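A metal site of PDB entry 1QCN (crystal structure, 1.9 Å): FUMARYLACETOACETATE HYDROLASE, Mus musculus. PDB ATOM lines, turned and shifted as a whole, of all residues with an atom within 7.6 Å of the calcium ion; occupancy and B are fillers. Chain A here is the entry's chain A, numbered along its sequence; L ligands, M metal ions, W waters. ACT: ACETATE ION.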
ATOM      1  N   TYR A 126       8.713  -4.653 -23.188  1.00  0.00           N
ATOM      2  CA  TYR A 126       9.581  -5.465 -22.338  1.00  0.00           C
ATOM      3  C   TYR A 126       9.581  -6.855 -22.968  1.00  0.00           C
ATOM      4  O   TYR A 126       8.526  -7.347 -23.379  1.00  0.00           O
ATOM      5  CB  TYR A 126       9.059  -5.491 -20.883  1.00  0.00           C
ATOM      6  CG  TYR A 126       9.377  -6.750 -20.060  1.00  0.00           C
ATOM      7  CD1 TYR A 126       8.357  -7.406 -19.354  1.00  0.00           C
ATOM      8  CD2 TYR A 126      10.654  -7.297 -20.028  1.00  0.00           C
ATOM      9  CE1 TYR A 126       8.601  -8.553 -18.639  1.00  0.00           C
ATOM     10  CE2 TYR A 126      10.920  -8.473 -19.302  1.00  0.00           C
ATOM     11  CZ  TYR A 126       9.877  -9.093 -18.613  1.00  0.00           C
ATOM     12  OH  TYR A 126      10.089 -10.274 -17.932  1.00  0.00           O
ATOM     13  N   ASP A 128      11.297 -10.873 -22.493  1.00  0.00           N
ATOM     14  CA  ASP A 128      12.039 -11.741 -21.599  1.00  0.00           C
ATOM     15  C   ASP A 128      12.620 -12.899 -22.389  1.00  0.00           C
ATOM     16  O   ASP A 128      11.872 -13.697 -22.961  1.00  0.00           O
ATOM     17  CB  ASP A 128      11.110 -12.286 -20.517  1.00  0.00           C
ATOM     18  CG  ASP A 128      11.858 -12.874 -19.350  1.00  0.00           C
ATOM     19  OD1 ASP A 128      12.879 -12.305 -18.952  1.00  0.00           O
ATOM     20  OD2 ASP A 128      11.418 -13.900 -18.820  1.00  0.00           O
ATOM     21  N   PHE A 129      13.950 -12.963 -22.479  1.00  0.00           N
ATOM     22  CA  PHE A 129      14.588 -14.061 -23.178  1.00  0.00           C
ATOM     23  C   PHE A 129      14.671 -15.289 -22.260  1.00  0.00           C
ATOM     24  O   PHE A 129      14.158 -15.244 -21.136  1.00  0.00           O
ATOM     25  CB  PHE A 129      15.936 -13.650 -23.781  1.00  0.00           C
ATOM     26  CG  PHE A 129      15.798 -12.752 -24.977  1.00  0.00           C
ATOM     27  CD1 PHE A 129      15.795 -11.366 -24.824  1.00  0.00           C
ATOM     28  CD2 PHE A 129      15.602 -13.283 -26.245  1.00  0.00           C
ATOM     29  CE1 PHE A 129      15.577 -10.519 -25.931  1.00  0.00           C
ATOM     30  CE2 PHE A 129      15.393 -12.450 -27.354  1.00  0.00           C
ATOM     31  CZ  PHE A 129      15.380 -11.064 -27.200  1.00  0.00           C
ATOM     32  N   TYR A 130      15.268 -16.369 -22.733  1.00  0.00           N
ATOM     33  CA  TYR A 130      15.338 -17.636 -21.981  1.00  0.00           C
ATOM     34  C   TYR A 130      16.739 -18.217 -22.261  1.00  0.00           C
ATOM     35  O   TYR A 130      16.902 -19.438 -22.475  1.00  0.00           O
ATOM     36  CB  TYR A 130      14.259 -18.554 -22.602  1.00  0.00           C
ATOM     37  CG  TYR A 130      13.759 -19.700 -21.775  1.00  0.00           C
ATOM     38  CD1 TYR A 130      13.556 -19.563 -20.403  1.00  0.00           C
ATOM     39  CD2 TYR A 130      13.435 -20.924 -22.372  1.00  0.00           C
ATOM     40  CE1 TYR A 130      13.035 -20.598 -19.660  1.00  0.00           C
ATOM     41  CE2 TYR A 130      12.904 -21.960 -21.628  1.00  0.00           C
ATOM     42  CZ  TYR A 130      12.709 -21.793 -20.268  1.00  0.00           C
ATOM     43  OH  TYR A 130      12.148 -22.795 -19.512  1.00  0.00           O
ATOM     44  N   HIS A 135      19.148 -23.199 -16.788  1.00  0.00           N
ATOM     45  CA  HIS A 135      17.789 -22.889 -16.366  1.00  0.00           C
ATOM     46  C   HIS A 135      16.807 -23.594 -17.274  1.00  0.00           C
ATOM     47  O   HIS A 135      15.898 -24.267 -16.799  1.00  0.00           O
ATOM     48  CB  HIS A 135      17.495 -21.393 -16.386  1.00  0.00           C
ATOM     49  CG  HIS A 135      16.067 -21.072 -16.063  1.00  0.00           C
ATOM     50  ND1 HIS A 135      15.553 -21.206 -14.793  1.00  0.00           N
ATOM     51  CD2 HIS A 135      15.029 -20.728 -16.863  1.00  0.00           C
ATOM     52  CE1 HIS A 135      14.256 -20.949 -14.821  1.00  0.00           C
ATOM     53  NE2 HIS A 135      13.913 -20.657 -16.059  1.00  0.00           N
ATOM     54  N   TYR A 161       9.908 -14.101 -25.183  1.00  0.00           N
ATOM     55  CA  TYR A 161       8.513 -13.744 -25.373  1.00  0.00           C
ATOM     56  C   TYR A 161       8.281 -12.283 -24.938  1.00  0.00           C
ATOM     57  O   TYR A 161       9.083 -11.729 -24.194  1.00  0.00           O
ATOM     58  CB  TYR A 161       7.582 -14.681 -24.572  1.00  0.00           C
ATOM     59  CG  TYR A 161       7.693 -14.565 -23.066  1.00  0.00           C
ATOM     60  CD1 TYR A 161       6.787 -13.787 -22.349  1.00  0.00           C
ATOM     61  CD2 TYR A 161       8.721 -15.200 -22.369  1.00  0.00           C
ATOM     62  CE1 TYR A 161       6.905 -13.627 -20.977  1.00  0.00           C
ATOM     63  CE2 TYR A 161       8.841 -15.061 -20.990  1.00  0.00           C
ATOM     64  CZ  TYR A 161       7.931 -14.267 -20.301  1.00  0.00           C
ATOM     65  OH  TYR A 161       8.068 -14.105 -18.944  1.00  0.00           O
ATOM     66  N   GLU A 201      12.462 -14.950  -9.833  1.00  0.00           N
ATOM     67  CA  GLU A 201      13.321 -15.350 -10.933  1.00  0.00           C
ATOM     68  C   GLU A 201      14.427 -14.323 -11.091  1.00  0.00           C
ATOM     69  O   GLU A 201      14.188 -13.153 -11.414  1.00  0.00           O
ATOM     70  CB  GLU A 201      12.555 -15.503 -12.246  1.00  0.00           C
ATOM     71  CG  GLU A 201      11.696 -16.763 -12.326  1.00  0.00           C
ATOM     72  CD  GLU A 201      11.259 -17.085 -13.736  1.00  0.00           C
ATOM     73  OE1 GLU A 201      11.086 -16.152 -14.522  1.00  0.00           O
ATOM     74  OE2 GLU A 201      11.109 -18.280 -14.062  1.00  0.00           O
ATOM     75  N   LEU A 202      15.637 -14.765 -10.761  1.00  0.00           N
ATOM     76  CA  LEU A 202      16.827 -13.939 -10.853  1.00  0.00           C
ATOM     77  C   LEU A 202      17.138 -13.656 -12.308  1.00  0.00           C
ATOM     78  O   LEU A 202      17.403 -14.584 -13.067  1.00  0.00           O
ATOM     79  CB  LEU A 202      18.015 -14.658 -10.197  1.00  0.00           C
ATOM     80  CG  LEU A 202      19.404 -14.033 -10.378  1.00  0.00           C
ATOM     81  CD1 LEU A 202      19.478 -12.721  -9.617  1.00  0.00           C
ATOM     82  CD2 LEU A 202      20.475 -14.986  -9.882  1.00  0.00           C
ATOM     83  N   GLU A 203      17.132 -12.384 -12.681  1.00  0.00           N
ATOM     84  CA  GLU A 203      17.428 -11.994 -14.043  1.00  0.00           C
ATOM     85  C   GLU A 203      18.184 -10.674 -14.078  1.00  0.00           C
ATOM     86  O   GLU A 203      18.345 -10.014 -13.054  1.00  0.00           O
ATOM     87  CB  GLU A 203      16.134 -11.821 -14.852  1.00  0.00           C
ATOM     88  CG  GLU A 203      15.184 -12.985 -14.796  1.00  0.00           C
ATOM     89  CD  GLU A 203      14.197 -12.993 -15.944  1.00  0.00           C
ATOM     90  OE1 GLU A 203      14.384 -12.235 -16.930  1.00  0.00           O
ATOM     91  OE2 GLU A 203      13.236 -13.777 -15.863  1.00  0.00           O
ATOM     92  N   MET A 233      16.788  -7.740 -12.189  1.00  0.00           N
ATOM     93  CA  MET A 233      15.357  -7.969 -12.328  1.00  0.00           C
ATOM     94  C   MET A 233      14.885  -9.210 -11.567  1.00  0.00           C
ATOM     95  O   MET A 233      15.613 -10.184 -11.433  1.00  0.00           O
ATOM     96  CB  MET A 233      14.968  -8.116 -13.803  1.00  0.00           C
ATOM     97  CG  MET A 233      13.503  -8.488 -14.041  1.00  0.00           C
ATOM     98  SD  MET A 233      13.040  -8.772 -15.831  1.00  0.00           S
ATOM     99  CE  MET A 233      12.891  -7.052 -16.390  1.00  0.00           C
ATOM    100  N   ASN A 234      13.676  -9.124 -11.009  1.00  0.00           N
ATOM    101  CA  ASN A 234      13.053 -10.265 -10.328  1.00  0.00           C
ATOM    102  C   ASN A 234      11.728 -10.480 -11.059  1.00  0.00           C
ATOM    103  O   ASN A 234      10.764  -9.717 -10.886  1.00  0.00           O
ATOM    104  CB  ASN A 234      12.805  -9.994  -8.843  1.00  0.00           C
ATOM    105  CG  ASN A 234      12.146 -11.180  -8.132  1.00  0.00           C
ATOM    106  OD1 ASN A 234      11.717 -12.134  -8.787  1.00  0.00           O
ATOM    107  ND2 ASN A 234      12.081 -11.134  -6.821  1.00  0.00           N
ATOM    108  N   ASP A 235      11.693 -11.464 -11.937  1.00  0.00           N
ATOM    109  CA  ASP A 235      10.490 -11.760 -12.685  1.00  0.00           C
ATOM    110  C   ASP A 235       9.592 -12.650 -11.834  1.00  0.00           C
ATOM    111  O   ASP A 235       9.623 -13.882 -11.951  1.00  0.00           O
ATOM    112  CB  ASP A 235      10.856 -12.435 -14.007  1.00  0.00           C
ATOM    113  CG  ASP A 235       9.657 -12.656 -14.914  1.00  0.00           C
ATOM    114  OD1 ASP A 235       8.593 -12.084 -14.687  1.00  0.00           O
ATOM    115  OD2 ASP A 235       9.786 -13.396 -15.884  1.00  0.00           O
ATOM    116  N   TRP A 236       8.806 -12.021 -10.953  1.00  0.00           N
ATOM    117  CA  TRP A 236       7.907 -12.737 -10.055  1.00  0.00           C
ATOM    118  C   TRP A 236       7.011 -13.665 -10.864  1.00  0.00           C
ATOM    119  O   TRP A 236       6.492 -13.284 -11.916  1.00  0.00           O
ATOM    120  CB  TRP A 236       7.063 -11.744  -9.237  1.00  0.00           C
ATOM    121  CG  TRP A 236       7.875 -10.747  -8.430  1.00  0.00           C
ATOM    122  CD1 TRP A 236       8.192  -9.460  -8.783  1.00  0.00           C
ATOM    123  CD2 TRP A 236       8.432 -10.947  -7.114  1.00  0.00           C
ATOM    124  NE1 TRP A 236       8.894  -8.848  -7.777  1.00  0.00           N
ATOM    125  CE2 TRP A 236       9.047  -9.728  -6.744  1.00  0.00           C
ATOM    126  CE3 TRP A 236       8.449 -12.027  -6.217  1.00  0.00           C
ATOM    127  CZ2 TRP A 236       9.686  -9.566  -5.498  1.00  0.00           C
ATOM    128  CZ3 TRP A 236       9.086 -11.864  -4.984  1.00  0.00           C
ATOM    129  CH2 TRP A 236       9.699 -10.644  -4.643  1.00  0.00           C
ATOM    130  N   SER A 237       6.845 -14.893 -10.386  1.00  0.00           N
ATOM    131  CA  SER A 237       6.072 -15.902 -11.091  1.00  0.00           C
ATOM    132  C   SER A 237       5.061 -16.669 -10.222  1.00  0.00           C
ATOM    133  O   SER A 237       5.346 -17.007  -9.074  1.00  0.00           O
ATOM    134  CB  SER A 237       7.036 -16.927 -11.701  1.00  0.00           C
ATOM    135  OG  SER A 237       8.215 -16.314 -12.218  1.00  0.00           O
ATOM    136  N   ARG A 239       3.646 -19.948 -10.543  1.00  0.00           N
ATOM    137  CA  ARG A 239       3.833 -21.198 -11.280  1.00  0.00           C
ATOM    138  C   ARG A 239       2.599 -22.035 -11.576  1.00  0.00           C
ATOM    139  O   ARG A 239       2.471 -22.612 -12.661  1.00  0.00           O
ATOM    140  CB  ARG A 239       4.869 -22.073 -10.585  1.00  0.00           C
ATOM    141  CG  ARG A 239       6.187 -21.368 -10.298  1.00  0.00           C
ATOM    142  CD  ARG A 239       6.894 -20.994 -11.578  1.00  0.00           C
ATOM    143  NE  ARG A 239       8.259 -20.549 -11.305  1.00  0.00           N
ATOM    144  CZ  ARG A 239       9.095 -20.088 -12.228  1.00  0.00           C
ATOM    145  NH1 ARG A 239       8.698 -20.023 -13.489  1.00  0.00           N
ATOM    146  NH2 ARG A 239      10.308 -19.674 -11.879  1.00  0.00           N
ATOM    147  N   GLN A 242       0.595 -20.154 -14.167  1.00  0.00           N
ATOM    148  CA  GLN A 242       1.360 -20.248 -15.411  1.00  0.00           C
ATOM    149  C   GLN A 242       1.192 -21.596 -16.108  1.00  0.00           C
ATOM    150  O   GLN A 242       0.886 -21.660 -17.300  1.00  0.00           O
ATOM    151  CB  GLN A 242       2.836 -20.001 -15.104  1.00  0.00           C
ATOM    152  CG  GLN A 242       3.693 -19.865 -16.355  1.00  0.00           C
ATOM    153  CD  GLN A 242       5.159 -19.583 -16.038  1.00  0.00           C
ATOM    154  OE1 GLN A 242       5.539 -19.402 -14.873  1.00  0.00           O
ATOM    155  NE2 GLN A 242       5.989 -19.534 -17.065  1.00  0.00           N
ATOM    156  N   PRO A 251       3.691 -17.632 -21.471  1.00  0.00           N
ATOM    157  CA  PRO A 251       3.525 -17.118 -20.099  1.00  0.00           C
ATOM    158  C   PRO A 251       2.641 -15.875 -20.194  1.00  0.00           C
ATOM    159  O   PRO A 251       2.898 -15.004 -21.030  1.00  0.00           O
ATOM    160  CB  PRO A 251       4.958 -16.774 -19.675  1.00  0.00           C
ATOM    161  CG  PRO A 251       5.808 -17.673 -20.508  1.00  0.00           C
ATOM    162  CD  PRO A 251       5.123 -17.617 -21.850  1.00  0.00           C
ATOM    163  N   LYS A 255       2.911 -14.213 -15.004  1.00  0.00           N
ATOM    164  CA  LYS A 255       4.075 -13.329 -15.012  1.00  0.00           C
ATOM    165  C   LYS A 255       3.740 -11.854 -14.837  1.00  0.00           C
ATOM    166  O   LYS A 255       4.493 -11.101 -14.225  1.00  0.00           O
ATOM    167  CB  LYS A 255       4.855 -13.454 -16.337  1.00  0.00           C
ATOM    168  CG  LYS A 255       5.098 -14.867 -16.841  1.00  0.00           C
ATOM    169  CD  LYS A 255       5.947 -15.680 -15.868  1.00  0.00           C
ATOM    170  CE  LYS A 255       7.317 -15.079 -15.707  1.00  0.00           C
ATOM    171  NZ  LYS A 255       8.242 -15.922 -14.900  1.00  0.00           N
ATOM    172  N   THR A 259       6.786  -7.364 -12.013  1.00  0.00           N
ATOM    173  CA  THR A 259       8.169  -7.662 -12.380  1.00  0.00           C
ATOM    174  C   THR A 259       8.974  -6.493 -11.817  1.00  0.00           C
ATOM    175  O   THR A 259       8.715  -5.344 -12.147  1.00  0.00           O
ATOM    176  CB  THR A 259       8.295  -7.761 -13.928  1.00  0.00           C
ATOM    177  OG1 THR A 259       7.422  -8.789 -14.411  1.00  0.00           O
ATOM    178  CG2 THR A 259       9.726  -8.091 -14.337  1.00  0.00           C
ATOM    179  N   ALA A 349      15.246  -8.611 -21.175  1.00  0.00           N
ATOM    180  CA  ALA A 349      15.755  -9.387 -20.055  1.00  0.00           C
ATOM    181  C   ALA A 349      16.356 -10.732 -20.467  1.00  0.00           C
ATOM    182  O   ALA A 349      15.993 -11.313 -21.481  1.00  0.00           O
ATOM    183  CB  ALA A 349      14.630  -9.573 -19.010  1.00  0.00           C
ATOM    184  N   SER A 350      17.262 -11.217 -19.627  1.00  0.00           N
ATOM    185  CA  SER A 350      17.988 -12.466 -19.838  1.00  0.00           C
ATOM    186  C   SER A 350      17.214 -13.775 -19.666  1.00  0.00           C
ATOM    187  O   SER A 350      17.534 -14.795 -20.294  1.00  0.00           O
ATOM    188  CB  SER A 350      19.163 -12.519 -18.861  1.00  0.00           C
ATOM    189  OG  SER A 350      18.681 -12.522 -17.522  1.00  0.00           O
ATOM    190  N   GLY A 351      16.216 -13.746 -18.803  1.00  0.00           N
ATOM    191  CA  GLY A 351      15.493 -14.951 -18.472  1.00  0.00           C
ATOM    192  C   GLY A 351      16.195 -15.392 -17.192  1.00  0.00           C
ATOM    193  O   GLY A 351      17.254 -14.862 -16.843  1.00  0.00           O
ATOM    194  N   THR A 352      15.590 -16.302 -16.447  1.00  0.00           N
ATOM    195  CA  THR A 352      16.180 -16.773 -15.201  1.00  0.00           C
ATOM    196  C   THR A 352      17.614 -17.244 -15.406  1.00  0.00           C
ATOM    197  O   THR A 352      17.901 -18.041 -16.309  1.00  0.00           O
ATOM    198  CB  THR A 352      15.346 -17.919 -14.621  1.00  0.00           C
ATOM    199  OG1 THR A 352      13.961 -17.570 -14.699  1.00  0.00           O
ATOM    200  CG2 THR A 352      15.726 -18.196 -13.187  1.00  0.00           C
HETATM  201  C   ACT L   1       9.369 -17.476 -17.814  1.00  0.00           C
HETATM  202  O   ACT L   1       9.524 -18.116 -18.901  1.00  0.00           O
HETATM  203  OXT ACT L   1       9.632 -16.281 -17.669  1.00  0.00           O
HETATM  204  CH3 ACT L   1       8.840 -18.259 -16.612  1.00  0.00           C
HETATM  205 CA    CA M   1      11.349 -14.969 -16.633  1.00  0.00          CA
HETATM  206  O   HOH W   1      12.690 -16.657 -17.548  1.00  0.00           O
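The backbone carbonyl oxygen of Asp 235 sits at hydrogen-bond distance from the side-chain hydroxyl of Ser 237 (2.8 Å).
OE1 of Glu 203 is in hydrogen-bond range of N of Gly 351, at 3.0 Å.
The backbone NH (N) of Met 233 lies within hydrogen-bond range of the backbone carbonyl oxygen (O) of Glu 203 (2.9 Å).
OG1 of Thr 352 sits close to OE2 of Glu 201 (3.0 Å).
The side-chain carboxylate (OE2) of Glu 201 lies within salt-bridge range of the guanidinium group (NH2) of Arg 239 (2.7 Å).
The backbone NH of Glu 201 is in hydrogen-bond range of the side-chain amide oxygen of Asn 234 (3.1 Å).
The backbone NH (N) of Asp 128 is in hydrogen-bond range of the backbone carbonyl oxygen (O) of Tyr 161 (2.9 Å).
The side-chain hydroxyl (OG) of Ser 237 sits at hydrogen-bond distance from the side-chain amino group (NZ) of Lys 255 (2.7 Å).
OD2 of Asp 235 is bound to the calcium ion (2.3 Å).
Water W1 binds the calcium ion.
OE2 of Glu 203 binds the calcium ion, 2.4 Å away.
The calcium ion is bound by an oxygen (OXT) of the ligand (2.4 Å).
The calcium ion is bound by OE1 of Glu 201, at 2.4 Å.
OD2 of Asp 128 is bound to the calcium ion (2.4 Å).
Residues that only touch the calcium ion: Lys 255 (3.7 Å).
Of the 23 residues printed, 5 come within 4 Å of the calcium ion.
Along chain A the residues within 4 Å of the calcium ion span positions 128 to 255.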
